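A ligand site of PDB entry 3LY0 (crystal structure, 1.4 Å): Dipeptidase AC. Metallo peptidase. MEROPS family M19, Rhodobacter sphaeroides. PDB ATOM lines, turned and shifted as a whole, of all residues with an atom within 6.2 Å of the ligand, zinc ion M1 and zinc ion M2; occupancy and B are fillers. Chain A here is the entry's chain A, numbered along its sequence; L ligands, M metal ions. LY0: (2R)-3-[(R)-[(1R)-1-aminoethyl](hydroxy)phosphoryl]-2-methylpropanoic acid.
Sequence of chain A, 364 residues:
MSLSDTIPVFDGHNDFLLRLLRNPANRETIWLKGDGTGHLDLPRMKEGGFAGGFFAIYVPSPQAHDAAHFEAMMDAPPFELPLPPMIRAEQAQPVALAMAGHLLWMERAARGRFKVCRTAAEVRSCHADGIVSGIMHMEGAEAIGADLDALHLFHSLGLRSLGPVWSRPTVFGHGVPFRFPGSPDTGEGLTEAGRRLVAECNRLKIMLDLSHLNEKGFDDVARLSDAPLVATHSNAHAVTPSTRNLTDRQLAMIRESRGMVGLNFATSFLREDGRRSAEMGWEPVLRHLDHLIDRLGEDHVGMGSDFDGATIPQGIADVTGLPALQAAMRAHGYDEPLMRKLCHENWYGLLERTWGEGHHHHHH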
ATOM      1  N   HIS A  13      -2.254  22.190  17.640  1.00  0.00           N
ATOM      2  CA  HIS A  13      -2.561  20.966  18.372  1.00  0.00           C
ATOM      3  C   HIS A  13      -1.932  20.899  19.751  1.00  0.00           C
ATOM      4  O   HIS A  13      -0.708  20.931  19.880  1.00  0.00           O
ATOM      5  CB  HIS A  13      -2.072  19.742  17.589  1.00  0.00           C
ATOM      6  CG  HIS A  13      -2.539  18.443  18.168  1.00  0.00           C
ATOM      7  ND1 HIS A  13      -3.745  17.872  17.811  1.00  0.00           N
ATOM      8  CD2 HIS A  13      -1.996  17.623  19.106  1.00  0.00           C
ATOM      9  CE1 HIS A  13      -3.898  16.737  18.466  1.00  0.00           C
ATOM     10  NE2 HIS A  13      -2.865  16.569  19.259  1.00  0.00           N
ATOM     11  N   ASN A  14      -2.763  20.760  20.790  1.00  0.00           N
ATOM     12  CA  ASN A  14      -2.213  20.433  22.112  1.00  0.00           C
ATOM     13  C   ASN A  14      -3.076  19.410  22.823  1.00  0.00           C
ATOM     14  O   ASN A  14      -4.259  19.267  22.512  1.00  0.00           O
ATOM     15  CB  ASN A  14      -2.015  21.689  22.979  1.00  0.00           C
ATOM     16  CG  ASN A  14      -3.300  22.171  23.637  1.00  0.00           C
ATOM     17  OD1 ASN A  14      -3.823  21.526  24.544  1.00  0.00           O
ATOM     18  ND2 ASN A  14      -3.795  23.310  23.176  1.00  0.00           N
ATOM     19  N   ASP A  15      -2.454  18.699  23.767  1.00  0.00           N
ATOM     20  CA  ASP A  15      -3.142  17.683  24.551  1.00  0.00           C
ATOM     21  C   ASP A  15      -3.279  18.056  26.023  1.00  0.00           C
ATOM     22  O   ASP A  15      -3.282  17.178  26.886  1.00  0.00           O
ATOM     23  CB  ASP A  15      -2.432  16.347  24.386  1.00  0.00           C
ATOM     24  CG  ASP A  15      -2.528  15.813  22.967  1.00  0.00           C
ATOM     25  OD1 ASP A  15      -3.655  15.484  22.529  1.00  0.00           O
ATOM     26  OD2 ASP A  15      -1.496  15.738  22.280  1.00  0.00           O
ATOM     27  N   LEU A  18      -5.682  16.091  28.198  1.00  0.00           N
ATOM     28  CA  LEU A  18      -5.306  14.796  28.735  1.00  0.00           C
ATOM     29  C   LEU A  18      -4.849  14.929  30.182  1.00  0.00           C
ATOM     30  O   LEU A  18      -5.041  14.031  31.003  1.00  0.00           O
ATOM     31  CB  LEU A  18      -4.210  14.156  27.868  1.00  0.00           C
ATOM     32  CG  LEU A  18      -3.810  12.715  28.199  1.00  0.00           C
ATOM     33  CD1 LEU A  18      -4.943  11.755  27.896  1.00  0.00           C
ATOM     34  CD2 LEU A  18      -2.564  12.351  27.382  1.00  0.00           C
ATOM     35  N   ALA A  56      -7.114  19.220  21.717  1.00  0.00           N
ATOM     36  CA  ALA A  56      -7.494  17.880  21.284  1.00  0.00           C
ATOM     37  C   ALA A  56      -8.180  17.068  22.360  1.00  0.00           C
ATOM     38  O   ALA A  56      -7.718  17.004  23.506  1.00  0.00           O
ATOM     39  CB  ALA A  56      -6.265  17.130  20.774  1.00  0.00           C
ATOM     40  N   TYR A  58      -8.571  13.344  22.843  1.00  0.00           N
ATOM     41  CA  TYR A  58      -7.916  12.141  22.360  1.00  0.00           C
ATOM     42  C   TYR A  58      -8.126  11.049  23.382  1.00  0.00           C
ATOM     43  O   TYR A  58      -7.888  11.272  24.572  1.00  0.00           O
ATOM     44  CB  TYR A  58      -6.425  12.414  22.123  1.00  0.00           C
ATOM     45  CG  TYR A  58      -5.492  11.287  22.491  1.00  0.00           C
ATOM     46  CD1 TYR A  58      -5.311  10.194  21.654  1.00  0.00           C
ATOM     47  CD2 TYR A  58      -4.770  11.335  23.672  1.00  0.00           C
ATOM     48  CE1 TYR A  58      -4.455   9.159  22.000  1.00  0.00           C
ATOM     49  CE2 TYR A  58      -3.906  10.318  24.029  1.00  0.00           C
ATOM     50  CZ  TYR A  58      -3.757   9.230  23.199  1.00  0.00           C
ATOM     51  OH  TYR A  58      -2.884   8.230  23.568  1.00  0.00           O
ATOM     52  N   HIS A  65       0.007   6.173  25.050  1.00  0.00           N
ATOM     53  CA  HIS A  65       1.101   6.590  24.169  1.00  0.00           C
ATOM     54  C   HIS A  65       2.399   6.824  24.916  1.00  0.00           C
ATOM     55  O   HIS A  65       3.482   6.653  24.352  1.00  0.00           O
ATOM     56  CB  HIS A  65       0.715   7.886  23.463  1.00  0.00           C
ATOM     57  CG  HIS A  65       0.625   9.059  24.393  1.00  0.00           C
ATOM     58  ND1 HIS A  65      -0.459   9.279  25.213  1.00  0.00           N
ATOM     59  CD2 HIS A  65       1.498  10.064  24.642  1.00  0.00           C
ATOM     60  CE1 HIS A  65      -0.253  10.369  25.921  1.00  0.00           C
ATOM     61  NE2 HIS A  65       0.921  10.869  25.598  1.00  0.00           N
ATOM     62  N   MET A  74      11.058   4.360  21.384  1.00  0.00           N
ATOM     63  CA  MET A  74      11.243   5.571  20.584  1.00  0.00           C
ATOM     64  C   MET A  74      12.569   6.283  20.884  1.00  0.00           C
ATOM     65  O   MET A  74      12.997   7.141  20.117  1.00  0.00           O
ATOM     66  CB  MET A  74      10.030   6.510  20.736  1.00  0.00           C
ATOM     67  CG  MET A  74       8.755   5.989  20.024  1.00  0.00           C
ATOM     68  SD  MET A  74       7.272   7.024  20.210  1.00  0.00           S
ATOM     69  CE  MET A  74       7.360   7.274  21.964  1.00  0.00           C
ATOM     70  N   GLU A 139      -9.207  14.100  18.149  1.00  0.00           N
ATOM     71  CA  GLU A 139      -8.071  13.424  17.543  1.00  0.00           C
ATOM     72  C   GLU A 139      -8.370  11.937  17.551  1.00  0.00           C
ATOM     73  O   GLU A 139      -8.142  11.271  18.563  1.00  0.00           O
ATOM     74  CB  GLU A 139      -6.795  13.705  18.345  1.00  0.00           C
ATOM     75  CG  GLU A 139      -5.572  12.952  17.827  1.00  0.00           C
ATOM     76  CD  GLU A 139      -4.275  13.431  18.466  1.00  0.00           C
ATOM     77  OE1 GLU A 139      -4.310  13.909  19.617  1.00  0.00           O
ATOM     78  OE2 GLU A 139      -3.220  13.335  17.828  1.00  0.00           O
ATOM     79  N   TRP A 166      -6.452   8.402  15.056  1.00  0.00           N
ATOM     80  CA  TRP A 166      -5.187   8.549  15.739  1.00  0.00           C
ATOM     81  C   TRP A 166      -4.314   7.423  15.165  1.00  0.00           C
ATOM     82  O   TRP A 166      -4.647   6.872  14.103  1.00  0.00           O
ATOM     83  CB  TRP A 166      -5.391   8.453  17.261  1.00  0.00           C
ATOM     84  CG  TRP A 166      -4.136   8.678  18.015  1.00  0.00           C
ATOM     85  CD1 TRP A 166      -3.397   9.832  18.076  1.00  0.00           C
ATOM     86  CD2 TRP A 166      -3.448   7.719  18.831  1.00  0.00           C
ATOM     87  NE1 TRP A 166      -2.289   9.640  18.870  1.00  0.00           N
ATOM     88  CE2 TRP A 166      -2.294   8.353  19.339  1.00  0.00           C
ATOM     89  CE3 TRP A 166      -3.690   6.381  19.176  1.00  0.00           C
ATOM     90  CZ2 TRP A 166      -1.380   7.700  20.175  1.00  0.00           C
ATOM     91  CZ3 TRP A 166      -2.770   5.736  20.003  1.00  0.00           C
ATOM     92  CH2 TRP A 166      -1.634   6.390  20.485  1.00  0.00           C
ATOM     93  N   SER A 167      -3.225   7.070  15.831  1.00  0.00           N
ATOM     94  CA  SER A 167      -2.377   5.968  15.342  1.00  0.00           C
ATOM     95  C   SER A 167      -2.942   4.635  15.836  1.00  0.00           C
ATOM     96  O   SER A 167      -2.329   3.946  16.665  1.00  0.00           O
ATOM     97  CB  SER A 167      -0.929   6.199  15.766  1.00  0.00           C
ATOM     98  OG  SER A 167      -0.319   7.192  14.943  1.00  0.00           O
ATOM     99  N   PHE A 178       3.612   4.170  14.861  1.00  0.00           N
ATOM    100  CA  PHE A 178       4.824   4.951  15.070  1.00  0.00           C
ATOM    101  C   PHE A 178       6.031   4.123  14.686  1.00  0.00           C
ATOM    102  O   PHE A 178       6.304   3.092  15.300  1.00  0.00           O
ATOM    103  CB  PHE A 178       4.937   5.385  16.531  1.00  0.00           C
ATOM    104  CG  PHE A 178       3.830   6.280  16.969  1.00  0.00           C
ATOM    105  CD1 PHE A 178       3.834   7.621  16.619  1.00  0.00           C
ATOM    106  CD2 PHE A 178       2.771   5.777  17.710  1.00  0.00           C
ATOM    107  CE1 PHE A 178       2.795   8.453  17.015  1.00  0.00           C
ATOM    108  CE2 PHE A 178       1.742   6.601  18.104  1.00  0.00           C
ATOM    109  CZ  PHE A 178       1.752   7.945  17.762  1.00  0.00           C
ATOM    110  N   SER A 211      -3.291  14.563  10.173  1.00  0.00           N
ATOM    111  CA  SER A 211      -2.232  14.035  11.039  1.00  0.00           C
ATOM    112  C   SER A 211      -2.671  12.690  11.623  1.00  0.00           C
ATOM    113  O   SER A 211      -3.784  12.554  12.148  1.00  0.00           O
ATOM    114  CB  SER A 211      -1.866  15.022  12.161  1.00  0.00           C
ATOM    115  OG  SER A 211      -1.243  16.197  11.646  1.00  0.00           O
ATOM    116  N   HIS A 212      -1.778  11.714  11.505  1.00  0.00           N
ATOM    117  CA  HIS A 212      -1.964  10.297  11.893  1.00  0.00           C
ATOM    118  C   HIS A 212      -2.548   9.418  10.827  1.00  0.00           C
ATOM    119  O   HIS A 212      -2.371   8.211  10.879  1.00  0.00           O
ATOM    120  CB  HIS A 212      -2.794  10.128  13.176  1.00  0.00           C
ATOM    121  CG  HIS A 212      -2.104  10.642  14.394  1.00  0.00           C
ATOM    122  ND1 HIS A 212      -1.218   9.876  15.123  1.00  0.00           N
ATOM    123  CD2 HIS A 212      -2.193  11.828  15.032  1.00  0.00           C
ATOM    124  CE1 HIS A 212      -0.759  10.596  16.137  1.00  0.00           C
ATOM    125  NE2 HIS A 212      -1.362  11.773  16.125  1.00  0.00           N
ATOM    126  N   HIS A 233      -0.380  18.721  12.968  1.00  0.00           N
ATOM    127  CA  HIS A 233       0.884  18.514  13.671  1.00  0.00           C
ATOM    128  C   HIS A 233       1.726  17.432  13.001  1.00  0.00           C
ATOM    129  O   HIS A 233       1.856  16.302  13.503  1.00  0.00           O
ATOM    130  CB  HIS A 233       0.675  18.310  15.202  1.00  0.00           C
ATOM    131  CG  HIS A 233      -0.186  17.136  15.590  1.00  0.00           C
ATOM    132  ND1 HIS A 233      -1.501  17.000  15.181  1.00  0.00           N
ATOM    133  CD2 HIS A 233       0.048  16.100  16.425  1.00  0.00           C
ATOM    134  CE1 HIS A 233      -2.006  15.901  15.704  1.00  0.00           C
ATOM    135  NE2 HIS A 233      -1.099  15.344  16.478  1.00  0.00           N
ATOM    136  N   ARG A 244       4.953   9.369  10.656  1.00  0.00           N
ATOM    137  CA  ARG A 244       4.040  10.468  11.004  1.00  0.00           C
ATOM    138  C   ARG A 244       4.199  11.722  10.132  1.00  0.00           C
ATOM    139  O   ARG A 244       3.337  12.606  10.157  1.00  0.00           O
ATOM    140  CB  ARG A 244       4.170  10.820  12.471  1.00  0.00           C
ATOM    141  CG  ARG A 244       3.308   9.943  13.371  1.00  0.00           C
ATOM    142  CD  ARG A 244       1.846  10.404  13.318  1.00  0.00           C
ATOM    143  NE  ARG A 244       1.611  11.574  14.164  1.00  0.00           N
ATOM    144  CZ  ARG A 244       1.416  12.821  13.726  1.00  0.00           C
ATOM    145  NH1 ARG A 244       1.452  13.112  12.433  1.00  0.00           N
ATOM    146  NH2 ARG A 244       1.166  13.780  14.605  1.00  0.00           N
ATOM    147  N   ASN A 264       5.085  20.200  14.081  1.00  0.00           N
ATOM    148  CA  ASN A 264       5.028  19.432  15.313  1.00  0.00           C
ATOM    149  C   ASN A 264       6.358  19.579  16.071  1.00  0.00           C
ATOM    150  O   ASN A 264       7.426  19.402  15.468  1.00  0.00           O
ATOM    151  CB  ASN A 264       4.742  17.970  14.961  1.00  0.00           C
ATOM    152  CG  ASN A 264       4.366  17.141  16.161  1.00  0.00           C
ATOM    153  OD1 ASN A 264       4.859  17.365  17.261  1.00  0.00           O
ATOM    154  ND2 ASN A 264       3.472  16.184  15.968  1.00  0.00           N
ATOM    155  N   ALA A 266       7.399  17.693  18.385  1.00  0.00           N
ATOM    156  CA  ALA A 266       7.888  16.392  18.857  1.00  0.00           C
ATOM    157  C   ALA A 266       9.294  16.116  18.350  1.00  0.00           C
ATOM    158  O   ALA A 266       9.537  16.152  17.143  1.00  0.00           O
ATOM    159  CB  ALA A 266       6.941  15.288  18.420  1.00  0.00           C
ATOM    160  N   PHE A 269       9.904  13.734  15.459  1.00  0.00           N
ATOM    161  CA  PHE A 269       9.467  14.090  14.107  1.00  0.00           C
ATOM    162  C   PHE A 269      10.283  15.239  13.535  1.00  0.00           C
ATOM    163  O   PHE A 269      10.086  15.609  12.380  1.00  0.00           O
ATOM    164  CB  PHE A 269       7.973  14.465  14.111  1.00  0.00           C
ATOM    165  CG  PHE A 269       7.079  13.398  14.693  1.00  0.00           C
ATOM    166  CD1 PHE A 269       7.456  12.062  14.699  1.00  0.00           C
ATOM    167  CD2 PHE A 269       5.841  13.748  15.228  1.00  0.00           C
ATOM    168  CE1 PHE A 269       6.622  11.084  15.244  1.00  0.00           C
ATOM    169  CE2 PHE A 269       4.997  12.785  15.759  1.00  0.00           C
ATOM    170  CZ  PHE A 269       5.385  11.457  15.780  1.00  0.00           C
ATOM    171  N   ASP A 306       1.987  20.173  19.547  1.00  0.00           N
ATOM    172  CA  ASP A 306       1.856  18.931  20.285  1.00  0.00           C
ATOM    173  C   ASP A 306       2.264  19.145  21.748  1.00  0.00           C
ATOM    174  O   ASP A 306       2.686  18.211  22.432  1.00  0.00           O
ATOM    175  CB  ASP A 306       2.703  17.812  19.658  1.00  0.00           C
ATOM    176  CG  ASP A 306       1.954  16.480  19.567  1.00  0.00           C
ATOM    177  OD1 ASP A 306       0.835  16.352  20.118  1.00  0.00           O
ATOM    178  OD2 ASP A 306       2.503  15.567  18.933  1.00  0.00           O
ATOM    179  N   ASP A 308       2.115  19.091  25.528  1.00  0.00           N
ATOM    180  CA  ASP A 308       1.536  18.107  26.446  1.00  0.00           C
ATOM    181  C   ASP A 308       1.200  16.749  25.816  1.00  0.00           C
ATOM    182  O   ASP A 308       0.618  15.877  26.472  1.00  0.00           O
ATOM    183  CB  ASP A 308       0.352  18.703  27.225  1.00  0.00           C
ATOM    184  CG  ASP A 308       0.819  19.593  28.369  1.00  0.00           C
ATOM    185  OD1 ASP A 308       1.817  19.224  29.028  1.00  0.00           O
ATOM    186  OD2 ASP A 308       0.199  20.651  28.610  1.00  0.00           O
ATOM    187  N   GLY A 309       1.604  16.568  24.560  1.00  0.00           N
ATOM    188  CA  GLY A 309       1.421  15.287  23.886  1.00  0.00           C
ATOM    189  C   GLY A 309       2.713  14.553  23.550  1.00  0.00           C
ATOM    190  O   GLY A 309       2.681  13.369  23.240  1.00  0.00           O
ATOM    191  N   ALA A 310       3.850  15.248  23.604  1.00  0.00           N
ATOM    192  CA  ALA A 310       5.125  14.682  23.174  1.00  0.00           C
ATOM    193  C   ALA A 310       6.294  15.374  23.856  1.00  0.00           C
ATOM    194  O   ALA A 310       6.148  16.471  24.382  1.00  0.00           O
ATOM    195  CB  ALA A 310       5.263  14.821  21.664  1.00  0.00           C
HETATM  196  P   LY0 L   1      -0.188  12.819  20.128  1.00  0.00           P
HETATM  197  C1  LY0 L   1      -0.681  11.012  22.206  1.00  0.00           C
HETATM  198  N1  LY0 L   1      -2.355  12.773  21.724  1.00  0.00           N
HETATM  199  C2  LY0 L   1      -0.940  12.431  21.746  1.00  0.00           C
HETATM  200  C4  LY0 L   1       1.640  12.770  20.244  1.00  0.00           C
HETATM  201  C5  LY0 L   1       2.335  11.987  19.177  1.00  0.00           C
HETATM  202  C6  LY0 L   1       1.825  12.302  17.792  1.00  0.00           C
HETATM  203  C7  LY0 L   1       3.837  11.957  19.301  1.00  0.00           C
HETATM  204  O31 LY0 L   1      -0.710  14.184  19.765  1.00  0.00           O
HETATM  205  O32 LY0 L   1      -0.720  11.790  19.067  1.00  0.00           O
HETATM  206  O61 LY0 L   1       2.157  11.475  16.768  1.00  0.00           O
HETATM  207  O62 LY0 L   1       1.097  13.284  17.572  1.00  0.00           O
HETATM  208 ZN    ZN M   1      -2.649  14.813  20.624  1.00  0.00          ZN
HETATM  209 ZN    ZN M   2      -1.144  13.394  17.585  1.00  0.00          ZN
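Zinc ion M2 is bound by the side-chain carboxylate of Glu 139, a ring nitrogen (NE2) of His 212, an oxygen (O32) of the ligand, a ring nitrogen (NE2) of His 233, an oxygen (O62) of the ligand and an oxygen (O31) of the ligand. Zinc ion M2 has six donor atoms within binding distance.
Tyr 58 touches the ligand. His 65 touches the ligand. Phe 178 touches the ligand (CE1 to O61, 3.1 Å). Phe 269 touches the ligand (CE2 to O61, 3.3 Å). Gly 309 touches the ligand. CB of Ala 310 touches C7 of the ligand (3.98 Å). 14 residues have an atom within 4 Å of the ligand: His 13, Asp 15, Tyr 58, His 65, Glu 139, Trp 166, Phe 178, His 212, His 233, Arg 244, Phe 269, Asp 306, Gly 309 and Ala 310.
Zinc ion M1 is bound by OE1 of Glu 139. An oxygen (O31) of the ligand is bound to zinc ion M1, 2.2 Å away. Zinc ion M1 is bound by OD2 of Asp 15 (2.2 Å). NE2 of His 13 is bound to zinc ion M1 (2.2 Å). Zinc ion M1 is bound by OD1 of Asp 15 (2.3 Å). N1 of the ligand binds zinc ion M1, 2.3 Å away.
Asp 306 touches zinc ion M1 (OD1 to ZN, 3.8 Å). Within 4 Å of zinc ion M1: His 13, Asp 15, Glu 139 and Asp 306. The nearest printed residue that does not touch zinc ion M1 is Ala 56 (4.3 Å).
Merely in contact with zinc ion M2: Arg 244. Within 4 Å of zinc ion M2: His 13, Glu 139, His 212, His 233 and Arg 244.
The guanidinium group (NE) of Arg 244 lies within salt-bridge range of an oxygen (O61) of the ligand, at 2.7 Å. NE1 of Trp 166 lies close to O32 of the ligand. OD1 of Asp 306 sits close to O31 of the ligand (2.7 Å).
The guanidinium group (NE) of Arg 244 sits close to a ring nitrogen (ND1) of His 212, at 3.4 Å. ND1 of His 212 is in hydrogen-bond range of OG of Ser 167 (2.8 Å). The backbone carbonyl oxygen (O) of His 13 is in hydrogen-bond range of the backbone NH (N) of Asp 306. The backbone carbonyl oxygen of His 233 lies within hydrogen-bond range of the guanidinium group of Arg 244. ND2 of Asn 264 is in hydrogen-bond range of O of His 233 (2.9 Å). N of His 233 sits at hydrogen-bond distance from OG of Ser 211 (3.0 Å). ND2 of Asn 264 sits at hydrogen-bond distance from OD2 of Asp 306. A ring nitrogen (ND1) of His 65 lies within hydrogen-bond range of the side-chain hydroxyl (OH) of Tyr 58 (3.1 Å).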
